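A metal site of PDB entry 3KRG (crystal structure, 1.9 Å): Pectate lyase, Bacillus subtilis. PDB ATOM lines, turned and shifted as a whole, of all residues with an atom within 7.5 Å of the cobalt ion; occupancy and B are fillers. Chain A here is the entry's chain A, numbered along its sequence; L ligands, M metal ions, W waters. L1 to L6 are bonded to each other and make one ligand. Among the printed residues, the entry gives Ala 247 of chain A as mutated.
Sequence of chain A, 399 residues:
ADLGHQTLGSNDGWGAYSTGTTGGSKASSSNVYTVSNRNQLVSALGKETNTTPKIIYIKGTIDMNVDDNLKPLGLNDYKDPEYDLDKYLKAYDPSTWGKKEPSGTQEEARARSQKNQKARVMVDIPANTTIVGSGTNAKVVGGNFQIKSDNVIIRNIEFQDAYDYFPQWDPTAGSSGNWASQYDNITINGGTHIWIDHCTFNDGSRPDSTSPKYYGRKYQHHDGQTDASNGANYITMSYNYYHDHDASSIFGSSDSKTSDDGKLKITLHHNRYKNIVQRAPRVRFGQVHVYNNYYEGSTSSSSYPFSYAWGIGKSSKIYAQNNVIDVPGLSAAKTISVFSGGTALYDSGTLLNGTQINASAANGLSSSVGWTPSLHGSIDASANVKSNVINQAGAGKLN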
ATOM      1  N   ASN A 144     -12.544  30.087  15.563  1.00  0.00           N
ATOM      2  CA  ASN A 144     -11.671  30.246  14.394  1.00  0.00           C
ATOM      3  C   ASN A 144     -12.190  31.517  13.714  1.00  0.00           C
ATOM      4  O   ASN A 144     -13.267  31.514  13.094  1.00  0.00           O
ATOM      5  CB  ASN A 144     -11.872  29.032  13.470  1.00  0.00           C
ATOM      6  CG  ASN A 144     -10.922  28.976  12.272  1.00  0.00           C
ATOM      7  OD1 ASN A 144     -10.822  27.919  11.633  1.00  0.00           O
ATOM      8  ND2 ASN A 144     -10.306  30.131  11.885  1.00  0.00           N
ATOM      9  N   SER A 181      -7.488  18.056  11.366  1.00  0.00           N
ATOM     10  CA  SER A 181      -8.626  18.841  11.802  1.00  0.00           C
ATOM     11  C   SER A 181      -8.709  20.170  11.036  1.00  0.00           C
ATOM     12  O   SER A 181      -7.789  20.501  10.283  1.00  0.00           O
ATOM     13  CB  SER A 181      -8.571  19.068  13.310  1.00  0.00           C
ATOM     14  OG  SER A 181      -9.005  17.859  13.947  1.00  0.00           O
ATOM     15  N   GLN A 182      -9.804  20.891  11.232  1.00  0.00           N
ATOM     16  CA  GLN A 182     -10.151  22.029  10.359  1.00  0.00           C
ATOM     17  C   GLN A 182      -9.946  23.430  10.930  1.00  0.00           C
ATOM     18  O   GLN A 182     -10.003  24.390  10.172  1.00  0.00           O
ATOM     19  CB  GLN A 182     -11.629  21.968  10.009  1.00  0.00           C
ATOM     20  CG  GLN A 182     -11.972  20.835   9.074  1.00  0.00           C
ATOM     21  CD  GLN A 182     -11.336  21.053   7.717  1.00  0.00           C
ATOM     22  OE1 GLN A 182     -11.692  21.996   6.996  1.00  0.00           O
ATOM     23  NE2 GLN A 182     -10.406  20.196   7.356  1.00  0.00           N
ATOM     24  N   TYR A 183      -9.832  23.572  12.264  1.00  0.00           N
ATOM     25  CA  TYR A 183      -9.948  24.946  12.816  1.00  0.00           C
ATOM     26  C   TYR A 183      -8.604  25.503  13.226  1.00  0.00           C
ATOM     27  O   TYR A 183      -7.899  24.851  14.006  1.00  0.00           O
ATOM     28  CB  TYR A 183     -10.923  24.957  14.029  1.00  0.00           C
ATOM     29  CG  TYR A 183     -12.216  24.285  13.645  1.00  0.00           C
ATOM     30  CD1 TYR A 183     -12.931  24.747  12.546  1.00  0.00           C
ATOM     31  CD2 TYR A 183     -12.660  23.132  14.294  1.00  0.00           C
ATOM     32  CE1 TYR A 183     -14.113  24.126  12.099  1.00  0.00           C
ATOM     33  CE2 TYR A 183     -13.868  22.486  13.881  1.00  0.00           C
ATOM     34  CZ  TYR A 183     -14.564  22.962  12.778  1.00  0.00           C
ATOM     35  OH  TYR A 183     -15.701  22.336  12.332  1.00  0.00           O
ATOM     36  N   ASP A 184      -8.274  26.709  12.717  1.00  0.00           N
ATOM     37  CA  ASP A 184      -7.124  27.499  13.186  1.00  0.00           C
ATOM     38  C   ASP A 184      -7.682  28.478  14.216  1.00  0.00           C
ATOM     39  O   ASP A 184      -8.892  28.640  14.328  1.00  0.00           O
ATOM     40  CB  ASP A 184      -6.564  28.365  12.045  1.00  0.00           C
ATOM     41  CG  ASP A 184      -6.132  27.533  10.838  1.00  0.00           C
ATOM     42  OD1 ASP A 184      -5.664  26.389  11.067  1.00  0.00           O
ATOM     43  OD2 ASP A 184      -6.255  28.029   9.676  1.00  0.00           O
ATOM     44  N   ASN A 185      -6.821  29.193  14.933  1.00  0.00           N
ATOM     45  CA  ASN A 185      -7.347  30.312  15.728  1.00  0.00           C
ATOM     46  C   ASN A 185      -7.777  31.470  14.824  1.00  0.00           C
ATOM     47  O   ASN A 185      -8.877  32.067  14.986  1.00  0.00           O
ATOM     48  CB  ASN A 185      -6.292  30.798  16.731  1.00  0.00           C
ATOM     49  CG  ASN A 185      -5.757  29.672  17.570  1.00  0.00           C
ATOM     50  OD1 ASN A 185      -4.620  29.254  17.373  1.00  0.00           O
ATOM     51  ND2 ASN A 185      -6.608  29.108  18.459  1.00  0.00           N
ATOM     52  N   ILE A 186      -6.908  31.756  13.862  1.00  0.00           N
ATOM     53  CA  ILE A 186      -7.190  32.754  12.836  1.00  0.00           C
ATOM     54  C   ILE A 186      -6.767  32.219  11.469  1.00  0.00           C
ATOM     55  O   ILE A 186      -5.633  31.821  11.313  1.00  0.00           O
ATOM     56  CB  ILE A 186      -6.409  34.103  13.087  1.00  0.00           C
ATOM     57  CG1 ILE A 186      -6.804  34.723  14.458  1.00  0.00           C
ATOM     58  CG2 ILE A 186      -6.659  35.133  11.861  1.00  0.00           C
ATOM     59  CD1 ILE A 186      -5.957  35.998  14.895  1.00  0.00           C
ATOM     60  N   THR A 187      -7.678  32.254  10.490  1.00  0.00           N
ATOM     61  CA  THR A 187      -7.371  31.864   9.130  1.00  0.00           C
ATOM     62  C   THR A 187      -7.536  33.080   8.236  1.00  0.00           C
ATOM     63  O   THR A 187      -8.617  33.640   8.177  1.00  0.00           O
ATOM     64  CB  THR A 187      -8.420  30.842   8.623  1.00  0.00           C
ATOM     65  OG1 THR A 187      -8.405  29.701   9.470  1.00  0.00           O
ATOM     66  CG2 THR A 187      -8.096  30.419   7.185  1.00  0.00           C
ATOM     67  N   ASP A 223      -5.439  22.475  14.327  1.00  0.00           N
ATOM     68  CA  ASP A 223      -4.771  22.688  13.064  1.00  0.00           C
ATOM     69  C   ASP A 223      -3.786  23.820  13.316  1.00  0.00           C
ATOM     70  O   ASP A 223      -2.879  23.719  14.167  1.00  0.00           O
ATOM     71  CB  ASP A 223      -5.787  22.989  11.927  1.00  0.00           C
ATOM     72  CG  ASP A 223      -5.101  22.949  10.521  1.00  0.00           C
ATOM     73  OD1 ASP A 223      -4.514  21.887  10.241  1.00  0.00           O
ATOM     74  OD2 ASP A 223      -5.124  23.942   9.721  1.00  0.00           O
ATOM     75  N   GLY A 224      -3.953  24.941  12.610  1.00  0.00           N
ATOM     76  CA  GLY A 224      -2.933  25.985  12.710  1.00  0.00           C
ATOM     77  C   GLY A 224      -3.271  27.025  13.771  1.00  0.00           C
ATOM     78  O   GLY A 224      -4.287  26.942  14.450  1.00  0.00           O
ATOM     79  N   GLN A 225      -2.394  28.008  13.942  1.00  0.00           N
ATOM     80  CA  GLN A 225      -2.664  29.141  14.826  1.00  0.00           C
ATOM     81  C   GLN A 225      -3.020  30.365  13.984  1.00  0.00           C
ATOM     82  O   GLN A 225      -4.160  30.886  14.057  1.00  0.00           O
ATOM     83  CB  GLN A 225      -1.426  29.391  15.720  1.00  0.00           C
ATOM     84  CG  GLN A 225      -1.163  28.185  16.615  1.00  0.00           C
ATOM     85  CD  GLN A 225       0.045  28.358  17.537  1.00  0.00           C
ATOM     86  OE1 GLN A 225       1.171  28.498  17.072  1.00  0.00           O
ATOM     87  NE2 GLN A 225      -0.196  28.359  18.838  1.00  0.00           N
ATOM     88  N   THR A 226      -2.073  30.849  13.173  1.00  0.00           N
ATOM     89  CA  THR A 226      -2.433  31.961  12.285  1.00  0.00           C
ATOM     90  C   THR A 226      -1.984  31.546  10.885  1.00  0.00           C
ATOM     91  O   THR A 226      -0.785  31.621  10.574  1.00  0.00           O
ATOM     92  CB  THR A 226      -1.723  33.294  12.705  1.00  0.00           C
ATOM     93  OG1 THR A 226      -0.342  33.030  13.011  1.00  0.00           O
ATOM     94  CG2 THR A 226      -2.380  33.894  13.929  1.00  0.00           C
ATOM     95  N   ASP A 227      -2.910  31.060  10.067  1.00  0.00           N
ATOM     96  CA  ASP A 227      -2.539  30.595   8.712  1.00  0.00           C
ATOM     97  C   ASP A 227      -2.995  31.611   7.667  1.00  0.00           C
ATOM     98  O   ASP A 227      -3.874  32.465   7.952  1.00  0.00           O
ATOM     99  CB  ASP A 227      -3.203  29.240   8.417  1.00  0.00           C
ATOM    100  CG  ASP A 227      -2.588  28.101   9.185  1.00  0.00           C
ATOM    101  OD1 ASP A 227      -1.455  28.173   9.724  1.00  0.00           O
ATOM    102  OD2 ASP A 227      -3.229  27.059   9.201  1.00  0.00           O
ATOM    103  N   ALA A 228      -2.365  31.609   6.487  1.00  0.00           N
ATOM    104  CA  ALA A 228      -2.706  32.575   5.435  1.00  0.00           C
ATOM    105  C   ALA A 228      -2.627  31.861   4.078  1.00  0.00           C
ATOM    106  O   ALA A 228      -1.665  31.180   3.803  1.00  0.00           O
ATOM    107  CB  ALA A 228      -1.752  33.814   5.481  1.00  0.00           C
ATOM    108  N   SER A 229      -3.657  32.044   3.271  1.00  0.00           N
ATOM    109  CA  SER A 229      -3.978  31.232   2.111  1.00  0.00           C
ATOM    110  C   SER A 229      -4.564  32.115   1.017  1.00  0.00           C
ATOM    111  O   SER A 229      -5.002  33.253   1.294  1.00  0.00           O
ATOM    112  CB  SER A 229      -5.140  30.304   2.522  1.00  0.00           C
ATOM    113  OG  SER A 229      -4.670  29.034   2.319  1.00  0.00           O
ATOM    114  N   ALA A 247       1.358  22.871  14.956  1.00  0.00           N
ATOM    115  CA  ALA A 247       1.653  23.570  13.683  1.00  0.00           C
ATOM    116  C   ALA A 247       1.237  25.030  13.757  1.00  0.00           C
ATOM    117  O   ALA A 247       0.053  25.311  13.835  1.00  0.00           O
ATOM    118  CB  ALA A 247       0.951  22.889  12.525  1.00  0.00           C
ATOM    119  N   SER A 248       2.175  25.969  13.761  1.00  0.00           N
ATOM    120  CA  SER A 248       1.791  27.395  14.045  1.00  0.00           C
ATOM    121  C   SER A 248       1.224  28.211  12.889  1.00  0.00           C
ATOM    122  O   SER A 248       0.093  28.688  12.937  1.00  0.00           O
ATOM    123  CB  SER A 248       2.969  28.168  14.652  1.00  0.00           C
ATOM    124  OG  SER A 248       2.609  29.541  14.785  1.00  0.00           O
ATOM    125  N   ILE A 250       1.078  28.468   8.517  1.00  0.00           N
ATOM    126  CA  ILE A 250       1.396  28.096   7.149  1.00  0.00           C
ATOM    127  C   ILE A 250       0.939  29.230   6.257  1.00  0.00           C
ATOM    128  O   ILE A 250      -0.236  29.647   6.324  1.00  0.00           O
ATOM    129  CB  ILE A 250       0.641  26.853   6.719  1.00  0.00           C
ATOM    130  CG1 ILE A 250       1.223  25.643   7.456  1.00  0.00           C
ATOM    131  CG2 ILE A 250       0.709  26.735   5.169  1.00  0.00           C
ATOM    132  CD1 ILE A 250       0.704  24.305   6.894  1.00  0.00           C
HETATM  133  C1  LIG L   1       4.273  17.349   7.316  1.00  0.00           C
HETATM  134  C2  LIG L   1       3.159  16.570   6.629  1.00  0.00           C
HETATM  135  C3  LIG L   1       3.439  16.268   5.179  1.00  0.00           C
HETATM  136  C4  LIG L   1       3.855  17.551   4.469  1.00  0.00           C
HETATM  137  C5  LIG L   1       5.083  18.178   5.105  1.00  0.00           C
HETATM  138  C6  LIG L   1       5.199  19.575   4.551  1.00  0.00           C
HETATM  139  O1  LIG L   1       5.278  16.445   7.755  1.00  0.00           O
HETATM  140  O2  LIG L   1       3.018  15.293   7.270  1.00  0.00           O
HETATM  141  O3  LIG L   1       2.198  15.766   4.679  1.00  0.00           O
HETATM  142  O4  LIG L   1       2.796  18.519   4.566  1.00  0.00           O
HETATM  143  O5  LIG L   1       4.892  18.367   6.510  1.00  0.00           O
HETATM  144  O6  LIG L   1       5.432  19.731   3.352  1.00  0.00           O
HETATM  145  O7  LIG L   1       5.024  20.578   5.294  1.00  0.00           O
HETATM  146  C1  LG2 L   2       1.555  18.409   4.023  1.00  0.00           C
HETATM  147  C2  LG2 L   2       1.502  19.689   3.188  1.00  0.00           C
HETATM  148  C3  LG2 L   2       1.250  20.934   4.046  1.00  0.00           C
HETATM  149  C4  LG2 L   2       0.026  20.678   4.911  1.00  0.00           C
HETATM  150  C5  LG2 L   2       0.229  19.382   5.698  1.00  0.00           C
HETATM  151  C6  LG2 L   2      -0.881  19.207   6.698  1.00  0.00           C
HETATM  152  O1  LG2 L   2       2.742  19.824   2.500  1.00  0.00           O
HETATM  153  O2  LG2 L   2       0.984  22.114   3.252  1.00  0.00           O
HETATM  154  O3  LG2 L   2      -1.068  20.506   4.022  1.00  0.00           O
HETATM  155  O4  LG2 L   2       0.334  18.275   4.787  1.00  0.00           O
HETATM  156  O5  LG2 L   2      -1.300  20.214   7.323  1.00  0.00           O
HETATM  157  O6  LG2 L   2      -1.330  18.061   6.864  1.00  0.00           O
HETATM  158  C1  LG3 L   3      -2.362  20.612   4.323  1.00  0.00           C
HETATM  159  C2  LG3 L   3      -3.459  20.362   3.318  1.00  0.00           C
HETATM  160  C3  LG3 L   3      -3.366  21.466   2.282  1.00  0.00           C
HETATM  161  C4  LG3 L   3      -3.587  22.804   2.966  1.00  0.00           C
HETATM  162  C5  LG3 L   3      -2.594  23.007   4.116  1.00  0.00           C
HETATM  163  C6  LG3 L   3      -2.967  24.187   4.978  1.00  0.00           C
HETATM  164  O1  LG3 L   3      -3.281  19.088   2.695  1.00  0.00           O
HETATM  165  O2  LG3 L   3      -4.362  21.277   1.286  1.00  0.00           O
HETATM  166  O3  LG3 L   3      -4.939  22.846   3.447  1.00  0.00           O
HETATM  167  O4  LG3 L   3      -2.635  21.854   4.970  1.00  0.00           O
HETATM  168  O5  LG3 L   3      -2.653  25.356   4.656  1.00  0.00           O
HETATM  169  O6  LG3 L   3      -3.592  23.939   6.042  1.00  0.00           O
HETATM  170  C1  LG4 L   4      -6.036  23.314   2.855  1.00  0.00           C
HETATM  171  C2  LG4 L   4      -7.507  22.953   3.121  1.00  0.00           C
HETATM  172  C3  LG4 L   4      -8.064  22.269   1.889  1.00  0.00           C
HETATM  173  C4  LG4 L   4      -7.988  23.307   0.796  1.00  0.00           C
HETATM  174  C5  LG4 L   4      -6.502  23.422   0.486  1.00  0.00           C
HETATM  175  C6  LG4 L   4      -6.315  24.220  -0.761  1.00  0.00           C
HETATM  176  O1  LG4 L   4      -7.595  22.046   4.216  1.00  0.00           O
HETATM  177  O2  LG4 L   4      -9.381  21.765   2.078  1.00  0.00           O
HETATM  178  O3  LG4 L   4      -8.499  24.576   1.259  1.00  0.00           O
HETATM  179  O4  LG4 L   4      -5.836  24.013   1.603  1.00  0.00           O
HETATM  180  O5  LG4 L   4      -6.907  23.832  -1.785  1.00  0.00           O
HETATM  181  O6  LG4 L   4      -5.564  25.221  -0.720  1.00  0.00           O
HETATM  182  C1  LG5 L   5      -9.482  24.883   0.404  1.00  0.00           C
HETATM  183  C2  LG5 L   5      -9.793  26.352   0.216  1.00  0.00           C
HETATM  184  C3  LG5 L   5     -10.114  26.937   1.581  1.00  0.00           C
HETATM  185  C4  LG5 L   5     -11.315  26.212   2.186  1.00  0.00           C
HETATM  186  C5  LG5 L   5     -10.984  24.722   2.230  1.00  0.00           C
HETATM  187  C6  LG5 L   5     -12.179  23.959   2.729  1.00  0.00           C
HETATM  188  O1  LG5 L   5      -8.628  26.972  -0.372  1.00  0.00           O
HETATM  189  O2  LG5 L   5     -10.421  28.316   1.483  1.00  0.00           O
HETATM  190  O3  LG5 L   5     -12.473  26.418   1.347  1.00  0.00           O
HETATM  191  O4  LG5 L   5     -10.645  24.244   0.928  1.00  0.00           O
HETATM  192  O5  LG5 L   5     -12.690  24.338   3.813  1.00  0.00           O
HETATM  193  O6  LG5 L   5     -12.607  22.989   2.048  1.00  0.00           O
HETATM  194  C1  LG6 L   6     -13.730  26.367   1.783  1.00  0.00           C
HETATM  195  C2  LG6 L   6     -14.925  26.135   0.863  1.00  0.00           C
HETATM  196  C3  LG6 L   6     -15.122  27.380   0.007  1.00  0.00           C
HETATM  197  C4  LG6 L   6     -15.068  28.693   0.804  1.00  0.00           C
HETATM  198  C5  LG6 L   6     -14.266  28.677   2.119  1.00  0.00           C
HETATM  199  C6  LG6 L   6     -14.897  29.608   3.141  1.00  0.00           C
HETATM  200  O1  LG6 L   6     -14.743  24.989   0.005  1.00  0.00           O
HETATM  201  O2  LG6 L   6     -16.367  27.217  -0.678  1.00  0.00           O
HETATM  202  O3  LG6 L   6     -16.410  29.146   1.055  1.00  0.00           O
HETATM  203  O4  LG6 L   6     -14.140  27.365   2.703  1.00  0.00           O
HETATM  204  O5  LG6 L   6     -15.157  30.784   2.786  1.00  0.00           O
HETATM  205  O6  LG6 L   6     -15.149  29.176   4.294  1.00  0.00           O
HETATM  206 CO    CO M   1      -5.251  26.106   8.831  1.00  0.00          CO
HETATM  207  O   HOH W   1      -7.470  25.418   8.504  1.00  0.00           O
HETATM  208  O   HOH W   2      -5.476  27.126   6.848  1.00  0.00           O
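The cobalt ion is bound by water W2 (2.2 Å). OD2 of Asp 227 is bound to the cobalt ion (2.3 Å). OD1 of Asp 184 is bound to the cobalt ion (2.3 Å). OD2 of Asp 184 binds the cobalt ion (2.3 Å). OD2 of Asp 223 is bound to the cobalt ion (2.3 Å). The cobalt ion is bound by water W1. The cobalt ion has six donor atoms within binding distance.
The side-chain carboxylate of Asp 184 lies close to the backbone NH of Gly 224 (2.7 Å). The side-chain amide oxygen (OD1) of Asn 144 lies within hydrogen-bond range of the backbone NH (N) of Asp 184, at 3.0 Å. O of Tyr 183 lies within hydrogen-bond range of N of Asp 223, 3.4 Å away. OD2 of Asp 184 sits close to OG1 of Thr 187, 2.7 Å away. The backbone carbonyl oxygen (O) of Ile 186 sits at hydrogen-bond distance from the backbone NH (N) of Asp 227 (3.1 Å). The side-chain carboxylate (OD1) of Asp 227 lies within hydrogen-bond range of the backbone NH (N) of Ile 250.
The nearest printed residue that does not touch the cobalt ion is Gly 224 (4.2 Å).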
